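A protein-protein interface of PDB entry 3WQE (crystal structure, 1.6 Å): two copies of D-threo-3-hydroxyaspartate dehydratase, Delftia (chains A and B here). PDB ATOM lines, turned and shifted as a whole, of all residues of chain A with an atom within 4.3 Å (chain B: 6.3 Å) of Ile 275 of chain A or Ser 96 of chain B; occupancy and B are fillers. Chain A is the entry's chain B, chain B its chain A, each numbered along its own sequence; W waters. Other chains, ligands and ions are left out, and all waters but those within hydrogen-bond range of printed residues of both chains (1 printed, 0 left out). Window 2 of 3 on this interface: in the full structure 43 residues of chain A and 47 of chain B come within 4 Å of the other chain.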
ATOM      1  N   THR A 273      15.734 -29.339 -13.437  1.00  0.00           N
ATOM      2  CA  THR A 273      14.827 -28.227 -13.146  1.00  0.00           C
ATOM      3  C   THR A 273      13.438 -28.748 -12.927  1.00  0.00           C
ATOM      4  O   THR A 273      12.986 -29.621 -13.689  1.00  0.00           O
ATOM      5  CB  THR A 273      14.831 -27.251 -14.379  1.00  0.00           C
ATOM      6  OG1 THR A 273      16.176 -26.742 -14.548  1.00  0.00           O
ATOM      7  CG2 THR A 273      13.892 -26.066 -14.129  1.00  0.00           C
ATOM      8  N   VAL A 274      12.705 -28.123 -11.973  1.00  0.00           N
ATOM      9  CA  VAL A 274      11.276 -28.404 -11.884  1.00  0.00           C
ATOM     10  C   VAL A 274      10.459 -27.720 -13.015  1.00  0.00           C
ATOM     11  O   VAL A 274      10.575 -26.515 -13.202  1.00  0.00           O
ATOM     12  CB  VAL A 274      10.724 -27.859 -10.571  1.00  0.00           C
ATOM     13  CG1 VAL A 274       9.217 -28.070 -10.423  1.00  0.00           C
ATOM     14  CG2 VAL A 274      11.418 -28.639  -9.455  1.00  0.00           C
ATOM     15  N   ILE A 275       9.731 -28.520 -13.789  1.00  0.00           N
ATOM     16  CA  ILE A 275       8.959 -28.002 -14.928  1.00  0.00           C
ATOM     17  C   ILE A 275       7.465 -28.143 -14.766  1.00  0.00           C
ATOM     18  O   ILE A 275       6.726 -27.645 -15.608  1.00  0.00           O
ATOM     19  CB  ILE A 275       9.377 -28.700 -16.227  1.00  0.00           C
ATOM     20  CG1 ILE A 275       9.170 -30.229 -16.143  1.00  0.00           C
ATOM     21  CG2 ILE A 275      10.865 -28.430 -16.523  1.00  0.00           C
ATOM     22  CD1 ILE A 275       9.456 -30.974 -17.487  1.00  0.00           C
ATOM     23  N   GLY A 276       6.982 -28.647 -13.617  1.00  0.00           N
ATOM     24  CA  GLY A 276       5.543 -28.703 -13.484  1.00  0.00           C
ATOM     25  C   GLY A 276       5.219 -29.430 -12.187  1.00  0.00           C
ATOM     26  O   GLY A 276       6.130 -29.817 -11.442  1.00  0.00           O
ATOM     27  N   ILE A 285       7.269 -32.337 -11.214  1.00  0.00           N
ATOM     28  CA  ILE A 285       7.804 -32.958 -12.429  1.00  0.00           C
ATOM     29  C   ILE A 285       9.109 -32.263 -12.733  1.00  0.00           C
ATOM     30  O   ILE A 285       9.124 -30.981 -12.724  1.00  0.00           O
ATOM     31  CB  ILE A 285       6.850 -32.753 -13.613  1.00  0.00           C
ATOM     32  CG1 ILE A 285       5.369 -33.059 -13.320  1.00  0.00           C
ATOM     33  CG2 ILE A 285       7.439 -33.513 -14.842  1.00  0.00           C
ATOM     34  CD1 ILE A 285       5.233 -34.437 -12.851  1.00  0.00           C
ATOM     35  N   VAL A 286      10.139 -33.053 -13.013  1.00  0.00           N
ATOM     36  CA  VAL A 286      11.437 -32.454 -13.306  1.00  0.00           C
ATOM     37  C   VAL A 286      11.876 -32.905 -14.688  1.00  0.00           C
ATOM     38  O   VAL A 286      11.298 -33.865 -15.250  1.00  0.00           O
ATOM     39  CB  VAL A 286      12.508 -32.868 -12.299  1.00  0.00           C
ATOM     40  CG1 VAL A 286      12.186 -32.236 -10.940  1.00  0.00           C
ATOM     41  CG2 VAL A 286      12.714 -34.415 -12.227  1.00  0.00           C
ATOM     42  N   ASP A 287      12.867 -32.189 -15.254  1.00  0.00           N
ATOM     43  CA  ASP A 287      13.375 -32.546 -16.568  1.00  0.00           C
ATOM     44  C   ASP A 287      14.462 -33.589 -16.618  1.00  0.00           C
ATOM     45  O   ASP A 287      15.151 -33.754 -17.681  1.00  0.00           O
ATOM     46  CB  ASP A 287      13.740 -31.276 -17.373  1.00  0.00           C
ATOM     47  CG  ASP A 287      14.936 -30.559 -16.752  1.00  0.00           C
ATOM     48  OD1 ASP A 287      15.487 -30.964 -15.714  1.00  0.00           O
ATOM     49  OD2 ASP A 287      15.259 -29.483 -17.294  1.00  0.00           O
ATOM     50  N   LEU A 351       8.165 -23.939  -9.610  1.00  0.00           N
ATOM     51  CA  LEU A 351       8.537 -24.061 -11.008  1.00  0.00           C
ATOM     52  C   LEU A 351       9.884 -23.340 -11.174  1.00  0.00           C
ATOM     53  O   LEU A 351      10.059 -22.224 -10.640  1.00  0.00           O
ATOM     54  CB  LEU A 351       7.445 -23.327 -11.863  1.00  0.00           C
ATOM     55  CG  LEU A 351       7.671 -23.194 -13.398  1.00  0.00           C
ATOM     56  CD1 LEU A 351       7.516 -24.576 -14.092  1.00  0.00           C
ATOM     57  CD2 LEU A 351       6.731 -22.157 -14.078  1.00  0.00           C
ATOM     58  N   TYR B  93       7.752 -29.236 -29.458  1.00  0.00           N
ATOM     59  CA  TYR B  93       8.566 -29.687 -28.302  1.00  0.00           C
ATOM     60  C   TYR B  93       7.599 -30.023 -27.219  1.00  0.00           C
ATOM     61  O   TYR B  93       7.032 -29.161 -26.541  1.00  0.00           O
ATOM     62  CB  TYR B  93       9.511 -28.532 -27.955  1.00  0.00           C
ATOM     63  CG  TYR B  93      10.251 -28.744 -26.678  1.00  0.00           C
ATOM     64  CD1 TYR B  93      10.722 -30.036 -26.335  1.00  0.00           C
ATOM     65  CD2 TYR B  93      10.501 -27.639 -25.820  1.00  0.00           C
ATOM     66  CE1 TYR B  93      11.431 -30.217 -25.103  1.00  0.00           C
ATOM     67  CE2 TYR B  93      11.193 -27.803 -24.625  1.00  0.00           C
ATOM     68  CZ  TYR B  93      11.645 -29.070 -24.295  1.00  0.00           C
ATOM     69  OH  TYR B  93      12.300 -29.258 -23.050  1.00  0.00           O
ATOM     70  N   ALA B  94       7.296 -31.338 -27.129  1.00  0.00           N
ATOM     71  CA  ALA B  94       6.195 -31.776 -26.295  1.00  0.00           C
ATOM     72  C   ALA B  94       6.638 -32.155 -24.886  1.00  0.00           C
ATOM     73  O   ALA B  94       6.325 -33.265 -24.403  1.00  0.00           O
ATOM     74  CB  ALA B  94       5.425 -32.948 -26.955  1.00  0.00           C
ATOM     75  N   VAL B  95       7.286 -31.230 -24.193  1.00  0.00           N
ATOM     76  CA  VAL B  95       7.666 -31.360 -22.723  1.00  0.00           C
ATOM     77  C   VAL B  95       7.394 -30.007 -22.138  1.00  0.00           C
ATOM     78  O   VAL B  95       7.836 -28.988 -22.704  1.00  0.00           O
ATOM     79  CB  VAL B  95       9.191 -31.758 -22.596  1.00  0.00           C
ATOM     80  CG1 VAL B  95       9.556 -31.732 -21.075  1.00  0.00           C
ATOM     81  CG2 VAL B  95       9.458 -33.136 -23.246  1.00  0.00           C
ATOM     82  N   SER B  96       6.695 -29.961 -21.003  1.00  0.00           N
ATOM     83  CA  SER B  96       6.307 -28.697 -20.416  1.00  0.00           C
ATOM     84  C   SER B  96       7.453 -27.741 -20.429  1.00  0.00           C
ATOM     85  O   SER B  96       8.562 -28.119 -19.967  1.00  0.00           O
ATOM     86  CB  SER B  96       6.088 -28.935 -18.953  1.00  0.00           C
ATOM     87  OG  SER B  96       4.939 -29.710 -18.823  1.00  0.00           O
ATOM     88  N   MET B  97       7.233 -26.523 -20.974  1.00  0.00           N
ATOM     89  CA  MET B  97       8.364 -25.643 -21.216  1.00  0.00           C
ATOM     90  C   MET B  97       8.992 -25.073 -19.895  1.00  0.00           C
ATOM     91  O   MET B  97       8.278 -24.542 -19.059  1.00  0.00           O
ATOM     92  CB  MET B  97       7.843 -24.473 -22.066  1.00  0.00           C
ATOM     93  CG  MET B  97       8.928 -23.449 -22.486  1.00  0.00           C
ATOM     94  SD  MET B  97      10.254 -24.308 -23.401  1.00  0.00           S
ATOM     95  CE  MET B  97      11.291 -22.796 -23.662  1.00  0.00           C
ATOM     96  N   ALA B  98      10.305 -25.197 -19.772  1.00  0.00           N
ATOM     97  CA  ALA B  98      11.043 -24.532 -18.678  1.00  0.00           C
ATOM     98  C   ALA B  98      11.421 -23.110 -19.091  1.00  0.00           C
ATOM     99  O   ALA B  98      12.015 -22.920 -20.142  1.00  0.00           O
ATOM    100  CB  ALA B  98      12.314 -25.320 -18.461  1.00  0.00           C
ATOM    101  N   HIS B 100      13.784 -21.150 -18.401  1.00  0.00           N
ATOM    102  CA  HIS B 100      15.174 -20.890 -18.659  1.00  0.00           C
ATOM    103  C   HIS B 100      15.558 -21.307 -20.064  1.00  0.00           C
ATOM    104  O   HIS B 100      16.564 -20.798 -20.537  1.00  0.00           O
ATOM    105  CB  HIS B 100      16.156 -21.511 -17.624  1.00  0.00           C
ATOM    106  CG  HIS B 100      16.362 -22.930 -17.785  1.00  0.00           C
ATOM    107  ND1 HIS B 100      15.607 -23.854 -17.145  1.00  0.00           N
ATOM    108  CD2 HIS B 100      17.261 -23.636 -18.566  1.00  0.00           C
ATOM    109  CE1 HIS B 100      16.042 -25.103 -17.501  1.00  0.00           C
ATOM    110  NE2 HIS B 100      17.075 -24.971 -18.342  1.00  0.00           N
ATOM    111  N   ARG B 101      14.736 -22.100 -20.731  1.00  0.00           N
ATOM    112  CA  ARG B 101      15.093 -22.506 -22.119  1.00  0.00           C
ATOM    113  C   ARG B 101      14.464 -21.515 -23.097  1.00  0.00           C
ATOM    114  O   ARG B 101      14.617 -21.744 -24.317  1.00  0.00           O
ATOM    115  CB  ARG B 101      14.573 -23.925 -22.388  1.00  0.00           C
ATOM    116  CG  ARG B 101      15.581 -24.971 -21.827  1.00  0.00           C
ATOM    117  CD  ARG B 101      15.263 -26.443 -22.253  1.00  0.00           C
ATOM    118  NE  ARG B 101      14.288 -27.113 -21.347  1.00  0.00           N
ATOM    119  CZ  ARG B 101      14.690 -27.768 -20.234  1.00  0.00           C
ATOM    120  NH1 ARG B 101      15.951 -27.764 -19.799  1.00  0.00           N
ATOM    121  NH2 ARG B 101      13.765 -28.360 -19.491  1.00  0.00           N
ATOM    122  N   ILE B 118       4.736 -26.289 -25.233  1.00  0.00           N
ATOM    123  CA  ILE B 118       3.543 -26.638 -24.469  1.00  0.00           C
ATOM    124  C   ILE B 118       3.639 -26.192 -23.028  1.00  0.00           C
ATOM    125  O   ILE B 118       4.755 -26.096 -22.450  1.00  0.00           O
ATOM    126  CB  ILE B 118       3.259 -28.175 -24.545  1.00  0.00           C
ATOM    127  CG1 ILE B 118       4.253 -29.062 -23.711  1.00  0.00           C
ATOM    128  CG2 ILE B 118       3.381 -28.690 -26.016  1.00  0.00           C
ATOM    129  CD1 ILE B 118       3.876 -30.564 -23.640  1.00  0.00           C
ATOM    130  N   VAL B 119       2.483 -25.984 -22.382  1.00  0.00           N
ATOM    131  CA  VAL B 119       2.482 -25.615 -20.933  1.00  0.00           C
ATOM    132  C   VAL B 119       1.261 -26.261 -20.279  1.00  0.00           C
ATOM    133  O   VAL B 119       0.288 -26.620 -20.976  1.00  0.00           O
ATOM    134  CB  VAL B 119       2.360 -24.107 -20.630  1.00  0.00           C
ATOM    135  CG1 VAL B 119       3.623 -23.363 -21.164  1.00  0.00           C
ATOM    136  CG2 VAL B 119       1.073 -23.479 -21.237  1.00  0.00           C
ATOM    137  N   ASP B 120       1.257 -26.344 -18.941  1.00  0.00           N
ATOM    138  CA  ASP B 120       0.081 -26.836 -18.221  1.00  0.00           C
ATOM    139  C   ASP B 120      -0.108 -26.013 -16.961  1.00  0.00           C
ATOM    140  O   ASP B 120      -0.872 -26.394 -16.038  1.00  0.00           O
ATOM    141  CB  ASP B 120       0.169 -28.322 -17.897  1.00  0.00           C
ATOM    142  CG  ASP B 120       1.311 -28.643 -16.938  1.00  0.00           C
ATOM    143  OD1 ASP B 120       2.027 -27.714 -16.464  1.00  0.00           O
ATOM    144  OD2 ASP B 120       1.450 -29.839 -16.570  1.00  0.00           O
ATOM    145  N   SER B 121       0.445 -24.796 -16.923  1.00  0.00           N
ATOM    146  CA  SER B 121       0.256 -23.913 -15.728  1.00  0.00           C
ATOM    147  C   SER B 121       0.170 -22.480 -16.122  1.00  0.00           C
ATOM    148  O   SER B 121       0.701 -22.073 -17.173  1.00  0.00           O
ATOM    149  CB  SER B 121       1.436 -24.158 -14.747  1.00  0.00           C
ATOM    150  OG  SER B 121       2.652 -23.626 -15.256  1.00  0.00           O
ATOM    151  N   ALA B 124       3.872 -20.957 -16.050  1.00  0.00           N
ATOM    152  CA  ALA B 124       4.696 -21.177 -17.261  1.00  0.00           C
ATOM    153  C   ALA B 124       4.125 -20.357 -18.445  1.00  0.00           C
ATOM    154  O   ALA B 124       4.890 -19.749 -19.228  1.00  0.00           O
ATOM    155  CB  ALA B 124       4.718 -22.618 -17.603  1.00  0.00           C
ATOM    156  N   GLU B 144      -1.278 -28.592 -22.477  1.00  0.00           N
ATOM    157  CA  GLU B 144      -1.238 -30.062 -22.300  1.00  0.00           C
ATOM    158  C   GLU B 144      -2.402 -30.457 -21.327  1.00  0.00           C
ATOM    159  O   GLU B 144      -2.588 -29.835 -20.286  1.00  0.00           O
ATOM    160  CB  GLU B 144       0.105 -30.491 -21.684  1.00  0.00           C
ATOM    161  CG  GLU B 144       0.205 -31.995 -21.647  1.00  0.00           C
ATOM    162  CD  GLU B 144       1.612 -32.497 -21.325  1.00  0.00           C
ATOM    163  OE1 GLU B 144       1.902 -33.641 -21.683  1.00  0.00           O
ATOM    164  OE2 GLU B 144       2.451 -31.761 -20.744  1.00  0.00           O
ATOM    165  N   SER B 152       1.899 -35.156 -16.989  1.00  0.00           N
ATOM    166  CA  SER B 152       1.607 -33.705 -16.955  1.00  0.00           C
ATOM    167  C   SER B 152       0.151 -33.449 -17.387  1.00  0.00           C
ATOM    168  O   SER B 152      -0.558 -34.364 -17.869  1.00  0.00           O
ATOM    169  CB  SER B 152       2.588 -32.800 -17.758  1.00  0.00           C
ATOM    170  OG  SER B 152       4.021 -33.037 -17.479  1.00  0.00           O
ATOM    171  N   GLY B 153      -0.292 -32.207 -17.148  1.00  0.00           N
ATOM    172  CA  GLY B 153      -1.427 -31.685 -17.818  1.00  0.00           C
ATOM    173  C   GLY B 153      -2.577 -31.173 -16.965  1.00  0.00           C
ATOM    174  O   GLY B 153      -2.807 -31.465 -15.780  1.00  0.00           O
HETATM  175  O   HOH W   1       6.208 -25.724 -17.499  1.00  0.00           O
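Water W1 lies within hydrogen-bond range of the backbone carbonyl oxygen (O) of Ile 275 of chain A (2.7 Å) and the backbone carbonyl oxygen (O) of Met 97 of chain B (2.8 Å).
NE of Arg 101 of chain B lies within hydrogen-bond range of OH of Tyr 93 of chain B, at 3.4 Å. The side-chain carboxylate of Asp 287 of chain A sits at hydrogen-bond distance from the backbone NH of Thr 273 of chain A, 2.8 Å away. The side-chain hydroxyl (OG) of Ser 121 of chain B lies within hydrogen-bond range of the backbone NH (N) of Ala 124 of chain B, 3.0 Å away. The backbone NH of Ile 275 of chain A sits at hydrogen-bond distance from the backbone carbonyl oxygen of Ile 285 of chain A (2.7 Å). NE2 of His 100 of chain B lies within hydrogen-bond range of NH1 of Arg 101 of chain B (3.3 Å).
Ile 275 of chain A touches just these residues of chain B: Val 95, Ser 96 and Ala 98. Ser 96 of chain B touches one residue of chain A. Of the printed residues of chain B, Thr 273 of chain A touches His 100. Printed residues of chain A within 4 Å of Arg 101 of chain B: Asp 287. Ile 285 of chain A touches none of the printed residues of chain B. Tyr 93 of chain B touches none of the printed residues of chain A. The nearest residue of chain B that does not touch Ile 275 of chain A is Arg 101 of chain B (4.2 Å). The nearest printed residue of chain B that does not touch Asp 287 of chain A is His 100 of chain B (4.5 Å).
Printed residues of chain A that touch a printed residue of chain B: Thr 273, Ile 275, Asp 287 and Leu 351. Hydrophobic or aromatic side chains of chain A within 4 Å of the printed part of chain B: Ile 275 and Leu 351. Printed residues of chain B that touch a printed residue of chain A: Val 95, Ser 96, Ala 98, His 100, Arg 101 and Ala 124. Hydrophobic or aromatic side chains of chain B within 4 Å of the printed part of chain A: Val 95, Ala 98 and His 100. Among the printed residues, Asp or Glu carboxylates within 4 Å of a Lys or Arg side-chain nitrogen of the other chain: Asp 287 of chain A with Arg 101 of chain B.
Among the printed residues, merely in contact across the chains: Thr 273 of chain A with His 100 of chain B (3.4 Å), Ile 275 of chain A with Ser 96 of chain B (3.6 Å), Ile 275 of chain A with Val 95 of chain B (3.7 Å), Leu 351 of chain A with Ala 124 of chain B (3.7 Å) and Ile 275 of chain A with Ala 98 of chain B (3.9 Å).
The guanidinium group (NH2) of Arg 101 of chain B lies within salt-bridge range of the side-chain carboxylate (OD2) of Asp 287 of chain A.
No position is printed for both chains. Of the 6 pairs that touch across the chains among the printed residues, none has its exchanged pair printed and touching as well.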
